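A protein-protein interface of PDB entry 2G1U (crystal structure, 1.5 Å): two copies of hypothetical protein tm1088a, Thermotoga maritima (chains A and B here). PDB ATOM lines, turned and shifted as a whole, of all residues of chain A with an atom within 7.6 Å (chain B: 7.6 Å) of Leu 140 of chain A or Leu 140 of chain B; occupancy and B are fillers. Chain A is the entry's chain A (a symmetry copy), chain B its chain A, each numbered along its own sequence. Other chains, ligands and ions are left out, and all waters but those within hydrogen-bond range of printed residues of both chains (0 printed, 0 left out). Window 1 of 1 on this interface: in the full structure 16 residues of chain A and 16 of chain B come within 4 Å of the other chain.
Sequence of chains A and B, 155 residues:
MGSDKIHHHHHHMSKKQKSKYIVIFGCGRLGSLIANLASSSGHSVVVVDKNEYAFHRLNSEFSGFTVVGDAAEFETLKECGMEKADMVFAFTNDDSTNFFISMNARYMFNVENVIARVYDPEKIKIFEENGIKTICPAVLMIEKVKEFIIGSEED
Leu 33 of chain A touches Ile 142 of chain B. Ile 135 of chain A touches Met 141 of chain B. Val 145 of chain B touches Ile 135 of chain A (CG2 to CD1, 3.7 Å). Leu 140 of chain A touches Leu 140 of chain B. Leu 140 of chain A touches Met 141 of chain B (CD2 to SD, 3.9 Å). CE of Met 141 of chain A touches CG2 of Ile 135 of chain B, 3.2 Å away. Leu 140 of chain B touches Met 141 of chain A. CG1 of Ile 142 of chain A touches CD2 of Leu 33 of chain B (3.7 Å). Ile 135 of chain B touches Val 145 of chain A.
Thr 134 of chain A touches none of the printed residues of chain B. Of the printed residues of chain B, Ile 135 of chain A touches Met 141 (3.2 Å) and Val 145 (3.7 Å). Printed residues of chain B within 4 Å of Leu 140 of chain A: Leu 140 (3.6 Å) and Met 141 (3.9 Å). Printed residues of chain B within 4 Å of Val 145 of chain A: Ile 135 (3.7 Å). Of the printed residues of chain A, Leu 33 of chain B touches Ile 142 (3.7 Å). Val 139 of chain B touches none of the printed residues of chain A. Printed residues of chain A within 4 Å of Leu 140 of chain B: Leu 140 (3.6 Å) and Met 141 (3.9 Å). Of the printed residues of chain A, Ile 142 of chain B touches Leu 33. The nearest printed residue of chain A that does not touch Leu 140 of chain B is Lys 144 of chain A (4.1 Å).
Hydrophobic or aromatic side chains of chain B that line the printed part of chain A: Leu 33, Ile 135, Leu 140, Met 141, Ile 142 and Val 145. Of the 16 printed residues of chain A, 6 touch a printed residue of chain B. Hydrophobic or aromatic side chains of chain A within 4 Å of the printed part of chain B: Leu 33, Ile 135, Leu 140, Met 141, Ile 142 and Val 145.
Leu 33 of chain A touches Ile 142 of chain B, and with the chains exchanged Ile 142 of chain A touches Leu 33 of chain B. Ile 135 of chain A touches Met 141 of chain B, and with the chains exchanged Met 141 of chain A touches Ile 135 of chain B. Leu 140 of chain A touches its own counterpart, Leu 140 of chain B. Leu 140 of chain A touches Met 141 of chain B, and with the chains exchanged Met 141 of chain A touches Leu 140 of chain B. Positions printed for both chains: 33, 124, 134, 135, 136, 137, 138, 139, 140, 141, 142, 143, 144, 145, 146 and 147.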
ATOM      1  N   LEU A  33     -27.825  15.742  13.705  1.00  0.00           N
ATOM      2  CA  LEU A  33     -26.505  15.183  13.433  1.00  0.00           C
ATOM      3  C   LEU A  33     -26.557  14.364  12.144  1.00  0.00           C
ATOM      4  O   LEU A  33     -25.670  14.491  11.273  1.00  0.00           O
ATOM      5  CB  LEU A  33     -26.101  14.309  14.615  1.00  0.00           C
ATOM      6  CG  LEU A  33     -24.792  13.552  14.686  1.00  0.00           C
ATOM      7  CD1 LEU A  33     -23.720  14.545  15.098  1.00  0.00           C
ATOM      8  CD2 LEU A  33     -24.834  12.435  15.712  1.00  0.00           C
ATOM      9  N   ILE A 124     -38.902  -2.643  21.233  1.00  0.00           N
ATOM     10  CA  ILE A 124     -38.095  -2.961  20.087  1.00  0.00           C
ATOM     11  C   ILE A 124     -38.748  -4.045  19.232  1.00  0.00           C
ATOM     12  O   ILE A 124     -38.767  -3.932  18.002  1.00  0.00           O
ATOM     13  CB  ILE A 124     -36.678  -3.403  20.510  1.00  0.00           C
ATOM     14  CG1 ILE A 124     -35.878  -2.215  21.060  1.00  0.00           C
ATOM     15  CG2 ILE A 124     -35.945  -4.101  19.361  1.00  0.00           C
ATOM     16  CD1 ILE A 124     -34.616  -2.592  21.830  1.00  0.00           C
ATOM     17  N   THR A 134     -33.911  -0.715  14.450  1.00  0.00           N
ATOM     18  CA  THR A 134     -34.031   0.091  15.667  1.00  0.00           C
ATOM     19  C   THR A 134     -32.702   0.568  16.212  1.00  0.00           C
ATOM     20  O   THR A 134     -31.697  -0.153  16.181  1.00  0.00           O
ATOM     21  CB  THR A 134     -34.788  -0.690  16.768  1.00  0.00           C
ATOM     22  OG1 THR A 134     -34.099  -1.909  17.105  1.00  0.00           O
ATOM     23  CG2 THR A 134     -36.190  -1.007  16.295  1.00  0.00           C
ATOM     24  N   ILE A 135     -32.725   1.772  16.757  1.00  0.00           N
ATOM     25  CA  ILE A 135     -31.617   2.283  17.532  1.00  0.00           C
ATOM     26  C   ILE A 135     -32.215   2.567  18.907  1.00  0.00           C
ATOM     27  O   ILE A 135     -33.012   3.506  19.076  1.00  0.00           O
ATOM     28  CB  ILE A 135     -31.054   3.558  16.958  1.00  0.00           C
ATOM     29  CG1 ILE A 135     -30.513   3.288  15.550  1.00  0.00           C
ATOM     30  CG2 ILE A 135     -29.963   4.129  17.883  1.00  0.00           C
ATOM     31  CD1 ILE A 135     -30.096   4.536  14.814  1.00  0.00           C
ATOM     32  N   CYS A 136     -31.825   1.776  19.879  1.00  0.00           N
ATOM     33  CA  CYS A 136     -32.275   1.956  21.267  1.00  0.00           C
ATOM     34  C   CYS A 136     -31.057   2.329  22.096  1.00  0.00           C
ATOM     35  O   CYS A 136     -30.154   1.527  22.271  1.00  0.00           O
ATOM     36  CB  CYS A 136     -32.897   0.680  21.792  1.00  0.00           C
ATOM     37  SG  CYS A 136     -33.294   0.732  23.550  1.00  0.00           S
ATOM     38  N   PRO A 137     -30.971   3.592  22.520  1.00  0.00           N
ATOM     39  CA  PRO A 137     -29.761   4.052  23.220  1.00  0.00           C
ATOM     40  C   PRO A 137     -29.306   3.176  24.374  1.00  0.00           C
ATOM     41  O   PRO A 137     -28.104   2.884  24.482  1.00  0.00           O
ATOM     42  CB  PRO A 137     -30.155   5.462  23.663  1.00  0.00           C
ATOM     43  CG  PRO A 137     -31.095   5.909  22.547  1.00  0.00           C
ATOM     44  CD  PRO A 137     -31.930   4.704  22.289  1.00  0.00           C
ATOM     45  N   ALA A 138     -30.219   2.756  25.252  1.00  0.00           N
ATOM     46  CA  ALA A 138     -29.812   1.929  26.390  1.00  0.00           C
ATOM     47  C   ALA A 138     -29.182   0.638  25.928  1.00  0.00           C
ATOM     48  O   ALA A 138     -28.183   0.188  26.493  1.00  0.00           O
ATOM     49  CB  ALA A 138     -30.971   1.658  27.289  1.00  0.00           C
ATOM     50  N   VAL A 139     -29.799   0.010  24.945  1.00  0.00           N
ATOM     51  CA  VAL A 139     -29.303  -1.283  24.434  1.00  0.00           C
ATOM     52  C   VAL A 139     -27.938  -1.098  23.783  1.00  0.00           C
ATOM     53  O   VAL A 139     -27.031  -1.923  23.985  1.00  0.00           O
ATOM     54  CB  VAL A 139     -30.326  -1.953  23.475  1.00  0.00           C
ATOM     55  CG1 VAL A 139     -29.706  -3.117  22.730  1.00  0.00           C
ATOM     56  CG2 VAL A 139     -31.486  -2.435  24.247  1.00  0.00           C
ATOM     57  N   LEU A 140     -27.792  -0.036  23.005  1.00  0.00           N
ATOM     58  CA  LEU A 140     -26.560   0.245  22.327  1.00  0.00           C
ATOM     59  C   LEU A 140     -25.384   0.467  23.320  1.00  0.00           C
ATOM     60  O   LEU A 140     -24.259  -0.035  23.110  1.00  0.00           O
ATOM     61  CB  LEU A 140     -26.769   1.453  21.439  1.00  0.00           C
ATOM     62  CG  LEU A 140     -25.773   1.735  20.338  1.00  0.00           C
ATOM     63  CD1 LEU A 140     -25.637   0.551  19.406  1.00  0.00           C
ATOM     64  CD2 LEU A 140     -26.187   2.963  19.570  1.00  0.00           C
ATOM     65  N   MET A 141     -25.652   1.196  24.409  1.00  0.00           N
ATOM     66  CA  MET A 141     -24.622   1.451  25.422  1.00  0.00           C
ATOM     67  C   MET A 141     -24.233   0.134  26.134  1.00  0.00           C
ATOM     68  O   MET A 141     -23.049  -0.166  26.290  1.00  0.00           O
ATOM     69  CB  MET A 141     -25.081   2.527  26.414  1.00  0.00           C
ATOM     70  CG  MET A 141     -25.541   3.837  25.759  1.00  0.00           C
ATOM     71  SD  MET A 141     -24.181   4.854  25.155  1.00  0.00           S
ATOM     72  CE  MET A 141     -23.266   5.095  26.684  1.00  0.00           C
ATOM     73  N   ILE A 142     -25.216  -0.659  26.538  1.00  0.00           N
ATOM     74  CA  ILE A 142     -24.957  -1.942  27.216  1.00  0.00           C
ATOM     75  C   ILE A 142     -24.193  -2.878  26.289  1.00  0.00           C
ATOM     76  O   ILE A 142     -23.238  -3.527  26.714  1.00  0.00           O
ATOM     77  CB  ILE A 142     -26.282  -2.602  27.661  1.00  0.00           C
ATOM     78  CG1 ILE A 142     -26.988  -1.810  28.789  1.00  0.00           C
ATOM     79  CG2 ILE A 142     -26.079  -4.057  28.083  1.00  0.00           C
ATOM     80  CD1 ILE A 142     -28.507  -2.215  28.975  1.00  0.00           C
ATOM     81  N   GLU A 143     -24.579  -2.931  25.016  1.00  0.00           N
ATOM     82  CA  GLU A 143     -23.875  -3.779  24.038  1.00  0.00           C
ATOM     83  C   GLU A 143     -22.395  -3.375  23.907  1.00  0.00           C
ATOM     84  O   GLU A 143     -21.533  -4.220  23.867  1.00  0.00           O
ATOM     85  CB  GLU A 143     -24.510  -3.695  22.651  1.00  0.00           C
ATOM     86  CG  GLU A 143     -25.743  -4.469  22.460  1.00  0.00           C
ATOM     87  CD  GLU A 143     -26.265  -4.330  21.023  1.00  0.00           C
ATOM     88  OE1 GLU A 143     -25.963  -3.299  20.334  1.00  0.00           O
ATOM     89  OE2 GLU A 143     -26.975  -5.265  20.596  1.00  0.00           O
ATOM     90  N   LYS A 144     -22.137  -2.077  23.884  1.00  0.00           N
ATOM     91  CA  LYS A 144     -20.768  -1.569  23.769  1.00  0.00           C
ATOM     92  C   LYS A 144     -19.966  -1.897  25.025  1.00  0.00           C
ATOM     93  O   LYS A 144     -18.829  -2.301  24.918  1.00  0.00           O
ATOM     94  CB  LYS A 144     -20.817  -0.063  23.507  1.00  0.00           C
ATOM     95  CG  LYS A 144     -19.467   0.558  23.177  1.00  0.00           C
ATOM     96  CD  LYS A 144     -18.907   0.001  21.898  1.00  0.00           C
ATOM     97  CE  LYS A 144     -17.786   0.883  21.341  1.00  0.00           C
ATOM     98  NZ  LYS A 144     -16.936   0.096  20.438  1.00  0.00           N
ATOM     99  N   VAL A 145     -20.547  -1.699  26.217  1.00  0.00           N
ATOM    100  CA  VAL A 145     -19.868  -2.096  27.460  1.00  0.00           C
ATOM    101  C   VAL A 145     -19.532  -3.588  27.419  1.00  0.00           C
ATOM    102  O   VAL A 145     -18.406  -4.023  27.741  1.00  0.00           O
ATOM    103  CB  VAL A 145     -20.702  -1.740  28.698  1.00  0.00           C
ATOM    104  CG1 VAL A 145     -20.179  -2.390  29.984  1.00  0.00           C
ATOM    105  CG2 VAL A 145     -20.761  -0.238  28.852  1.00  0.00           C
ATOM    106  N   LYS A 146     -20.509  -4.399  27.019  1.00  0.00           N
ATOM    107  CA  LYS A 146     -20.246  -5.838  26.954  1.00  0.00           C
ATOM    108  C   LYS A 146     -19.083  -6.164  26.024  1.00  0.00           C
ATOM    109  O   LYS A 146     -18.264  -7.018  26.350  1.00  0.00           O
ATOM    110  CB  LYS A 146     -21.474  -6.613  26.498  1.00  0.00           C
ATOM    111  CG  LYS A 146     -22.468  -6.823  27.612  1.00  0.00           C
ATOM    112  CD  LYS A 146     -23.327  -8.059  27.378  1.00  0.00           C
ATOM    113  CE  LYS A 146     -24.367  -8.226  28.485  1.00  0.00           C
ATOM    114  N   GLU A 147     -19.015  -5.526  24.852  1.00  0.00           N
ATOM    115  CA  GLU A 147     -17.912  -5.770  23.919  1.00  0.00           C
ATOM    116  C   GLU A 147     -16.596  -5.471  24.552  1.00  0.00           C
ATOM    117  O   GLU A 147     -15.624  -6.192  24.320  1.00  0.00           O
ATOM    118  CB  GLU A 147     -18.019  -4.946  22.636  1.00  0.00           C
ATOM    119  CG  GLU A 147     -19.133  -5.350  21.751  1.00  0.00           C
ATOM    120  CD  GLU A 147     -19.119  -4.613  20.404  1.00  0.00           C
ATOM    121  OE1 GLU A 147     -18.304  -3.661  20.236  1.00  0.00           O
ATOM    122  OE2 GLU A 147     -19.931  -5.006  19.522  1.00  0.00           O
ATOM    123  N   LEU B  33     -27.630   2.342  35.122  1.00  0.00           N
ATOM    124  CA  LEU B  33     -28.002   1.187  34.312  1.00  0.00           C
ATOM    125  C   LEU B  33     -26.911   0.123  34.414  1.00  0.00           C
ATOM    126  O   LEU B  33     -27.205  -1.075  34.610  1.00  0.00           O
ATOM    127  CB  LEU B  33     -28.178   1.648  32.870  1.00  0.00           C
ATOM    128  CG  LEU B  33     -28.556   0.720  31.736  1.00  0.00           C
ATOM    129  CD1 LEU B  33     -30.056   0.502  31.813  1.00  0.00           C
ATOM    130  CD2 LEU B  33     -28.224   1.312  30.379  1.00  0.00           C
ATOM    131  N   ILE B 124     -11.675  11.900  22.027  1.00  0.00           N
ATOM    132  CA  ILE B 124     -11.518  10.472  22.072  1.00  0.00           C
ATOM    133  C   ILE B 124     -10.046  10.074  21.991  1.00  0.00           C
ATOM    134  O   ILE B 124      -9.604   9.195  22.739  1.00  0.00           O
ATOM    135  CB  ILE B 124     -12.313   9.789  20.939  1.00  0.00           C
ATOM    136  CG1 ILE B 124     -13.822   9.885  21.198  1.00  0.00           C
ATOM    137  CG2 ILE B 124     -11.860   8.341  20.735  1.00  0.00           C
ATOM    138  CD1 ILE B 124     -14.702   9.570  19.992  1.00  0.00           C
ATOM    139  N   THR B 134     -13.352   3.974  25.026  1.00  0.00           N
ATOM    140  CA  THR B 134     -14.296   5.094  25.024  1.00  0.00           C
ATOM    141  C   THR B 134     -15.681   4.718  24.543  1.00  0.00           C
ATOM    142  O   THR B 134     -15.845   3.918  23.614  1.00  0.00           O
ATOM    143  CB  THR B 134     -13.755   6.264  24.168  1.00  0.00           C
ATOM    144  OG1 THR B 134     -13.543   5.854  22.804  1.00  0.00           O
ATOM    145  CG2 THR B 134     -12.456   6.769  24.759  1.00  0.00           C
ATOM    146  N   ILE B 135     -16.671   5.347  25.154  1.00  0.00           N
ATOM    147  CA  ILE B 135     -18.030   5.291  24.666  1.00  0.00           C
ATOM    148  C   ILE B 135     -18.394   6.747  24.388  1.00  0.00           C
ATOM    149  O   ILE B 135     -18.561   7.553  25.319  1.00  0.00           O
ATOM    150  CB  ILE B 135     -18.984   4.723  25.686  1.00  0.00           C
ATOM    151  CG1 ILE B 135     -18.580   3.282  26.014  1.00  0.00           C
ATOM    152  CG2 ILE B 135     -20.433   4.800  25.169  1.00  0.00           C
ATOM    153  CD1 ILE B 135     -19.356   2.684  27.160  1.00  0.00           C
ATOM    154  N   CYS B 136     -18.529   7.076  23.125  1.00  0.00           N
ATOM    155  CA  CYS B 136     -18.925   8.428  22.702  1.00  0.00           C
ATOM    156  C   CYS B 136     -20.287   8.316  22.039  1.00  0.00           C
ATOM    157  O   CYS B 136     -20.418   7.720  20.981  1.00  0.00           O
ATOM    158  CB  CYS B 136     -17.912   8.997  21.732  1.00  0.00           C
ATOM    159  SG  CYS B 136     -18.411  10.566  20.997  1.00  0.00           S
ATOM    160  N   PRO B 137     -21.335   8.794  22.713  1.00  0.00           N
ATOM    161  CA  PRO B 137     -22.696   8.608  22.185  1.00  0.00           C
ATOM    162  C   PRO B 137     -22.892   9.015  20.735  1.00  0.00           C
ATOM    163  O   PRO B 137     -23.519   8.264  19.970  1.00  0.00           O
ATOM    164  CB  PRO B 137     -23.540   9.437  23.155  1.00  0.00           C
ATOM    165  CG  PRO B 137     -22.770   9.299  24.465  1.00  0.00           C
ATOM    166  CD  PRO B 137     -21.348   9.440  24.052  1.00  0.00           C
ATOM    167  N   ALA B 138     -22.393  10.184  20.330  1.00  0.00           N
ATOM    168  CA  ALA B 138     -22.584  10.619  18.945  1.00  0.00           C
ATOM    169  C   ALA B 138     -21.961   9.643  17.977  1.00  0.00           C
ATOM    170  O   ALA B 138     -22.541   9.334  16.934  1.00  0.00           O
ATOM    171  CB  ALA B 138     -22.032  11.990  18.739  1.00  0.00           C
ATOM    172  N   VAL B 139     -20.755   9.206  18.288  1.00  0.00           N
ATOM    173  CA  VAL B 139     -20.026   8.279  17.400  1.00  0.00           C
ATOM    174  C   VAL B 139     -20.755   6.944  17.325  1.00  0.00           C
ATOM    175  O   VAL B 139     -20.884   6.361  16.235  1.00  0.00           O
ATOM    176  CB  VAL B 139     -18.542   8.116  17.833  1.00  0.00           C
ATOM    177  CG1 VAL B 139     -17.879   6.959  17.115  1.00  0.00           C
ATOM    178  CG2 VAL B 139     -17.800   9.357  17.540  1.00  0.00           C
ATOM    179  N   LEU B 140     -21.219   6.459  18.467  1.00  0.00           N
ATOM    180  CA  LEU B 140     -21.914   5.206  18.531  1.00  0.00           C
ATOM    181  C   LEU B 140     -23.219   5.216  17.686  1.00  0.00           C
ATOM    182  O   LEU B 140     -23.529   4.244  16.965  1.00  0.00           O
ATOM    183  CB  LEU B 140     -22.200   4.894  19.985  1.00  0.00           C
ATOM    184  CG  LEU B 140     -22.572   3.482  20.374  1.00  0.00           C
ATOM    185  CD1 LEU B 140     -21.509   2.497  19.938  1.00  0.00           C
ATOM    186  CD2 LEU B 140     -22.788   3.396  21.861  1.00  0.00           C
ATOM    187  N   MET B 141     -23.965   6.325  17.755  1.00  0.00           N
ATOM    188  CA  MET B 141     -25.207   6.451  16.982  1.00  0.00           C
ATOM    189  C   MET B 141     -24.893   6.496  15.468  1.00  0.00           C
ATOM    190  O   MET B 141     -25.522   5.791  14.679  1.00  0.00           O
ATOM    191  CB  MET B 141     -26.016   7.671  17.439  1.00  0.00           C
ATOM    192  CG  MET B 141     -26.303   7.713  18.946  1.00  0.00           C
ATOM    193  SD  MET B 141     -27.588   6.561  19.465  1.00  0.00           S
ATOM    194  CE  MET B 141     -28.957   7.141  18.454  1.00  0.00           C
ATOM    195  N   ILE B 142     -23.913   7.295  15.068  1.00  0.00           N
ATOM    196  CA  ILE B 142     -23.524   7.405  13.651  1.00  0.00           C
ATOM    197  C   ILE B 142     -23.027   6.060  13.139  1.00  0.00           C
ATOM    198  O   ILE B 142     -23.393   5.642  12.041  1.00  0.00           O
ATOM    199  CB  ILE B 142     -22.428   8.480  13.467  1.00  0.00           C
ATOM    200  CG1 ILE B 142     -22.951   9.911  13.741  1.00  0.00           C
ATOM    201  CG2 ILE B 142     -21.786   8.407  12.081  1.00  0.00           C
ATOM    202  CD1 ILE B 142     -21.789  10.964  13.964  1.00  0.00           C
ATOM    203  N   GLU B 143     -22.225   5.359  13.936  1.00  0.00           N
ATOM    204  CA  GLU B 143     -21.725   4.029  13.541  1.00  0.00           C
ATOM    205  C   GLU B 143     -22.884   3.042  13.305  1.00  0.00           C
ATOM    206  O   GLU B 143     -22.872   2.306  12.347  1.00  0.00           O
ATOM    207  CB  GLU B 143     -20.805   3.428  14.602  1.00  0.00           C
ATOM    208  CG  GLU B 143     -19.434   3.953  14.635  1.00  0.00           C
ATOM    209  CD  GLU B 143     -18.601   3.251  15.718  1.00  0.00           C
ATOM    210  OE1 GLU B 143     -19.182   2.724  16.725  1.00  0.00           O
ATOM    211  OE2 GLU B 143     -17.364   3.232  15.543  1.00  0.00           O
ATOM    212  N   LYS B 144     -23.882   3.084  14.172  1.00  0.00           N
ATOM    213  CA  LYS B 144     -25.042   2.199  14.049  1.00  0.00           C
ATOM    214  C   LYS B 144     -25.858   2.552  12.809  1.00  0.00           C
ATOM    215  O   LYS B 144     -26.282   1.664  12.101  1.00  0.00           O
ATOM    216  CB  LYS B 144     -25.881   2.300  15.324  1.00  0.00           C
ATOM    217  CG  LYS B 144     -27.015   1.287  15.408  1.00  0.00           C
ATOM    218  CD  LYS B 144     -26.489  -0.120  15.448  1.00  0.00           C
ATOM    219  CE  LYS B 144     -27.553  -1.107  15.939  1.00  0.00           C
ATOM    220  NZ  LYS B 144     -27.218  -2.464  15.490  1.00  0.00           N
ATOM    221  N   VAL B 145     -26.102   3.846  12.558  1.00  0.00           N
ATOM    222  CA  VAL B 145     -26.788   4.257  11.324  1.00  0.00           C
ATOM    223  C   VAL B 145     -26.019   3.748  10.103  1.00  0.00           C
ATOM    224  O   VAL B 145     -26.591   3.180   9.149  1.00  0.00           O
ATOM    225  CB  VAL B 145     -26.991   5.777  11.269  1.00  0.00           C
ATOM    226  CG1 VAL B 145     -27.431   6.277   9.889  1.00  0.00           C
ATOM    227  CG2 VAL B 145     -27.991   6.191  12.324  1.00  0.00           C
ATOM    228  N   LYS B 146     -24.702   3.944  10.115  1.00  0.00           N
ATOM    229  CA  LYS B 146     -23.910   3.475   8.977  1.00  0.00           C
ATOM    230  C   LYS B 146     -24.065   1.974   8.755  1.00  0.00           C
ATOM    231  O   LYS B 146     -24.169   1.535   7.613  1.00  0.00           O
ATOM    232  CB  LYS B 146     -22.434   3.799   9.148  1.00  0.00           C
ATOM    233  CG  LYS B 146     -22.115   5.233   8.806  1.00  0.00           C
ATOM    234  CD  LYS B 146     -20.667   5.401   8.367  1.00  0.00           C
ATOM    235  CE  LYS B 146     -20.344   6.866   8.079  1.00  0.00           C
ATOM    236  N   GLU B 147     -24.043   1.174   9.824  1.00  0.00           N
ATOM    237  CA  GLU B 147     -24.210  -0.276   9.689  1.00  0.00           C
ATOM    238  C   GLU B 147     -25.507  -0.609   9.035  1.00  0.00           C
ATOM    239  O   GLU B 147     -25.568  -1.537   8.227  1.00  0.00           O
ATOM    240  CB  GLU B 147     -24.151  -1.012  11.027  1.00  0.00           C
ATOM    241  CG  GLU B 147     -22.812  -1.016  11.655  1.00  0.00           C
ATOM    242  CD  GLU B 147     -22.748  -1.893  12.913  1.00  0.00           C
ATOM    243  OE1 GLU B 147     -23.819  -2.381  13.374  1.00  0.00           O
ATOM    244  OE2 GLU B 147     -21.611  -2.089  13.425  1.00  0.00           O
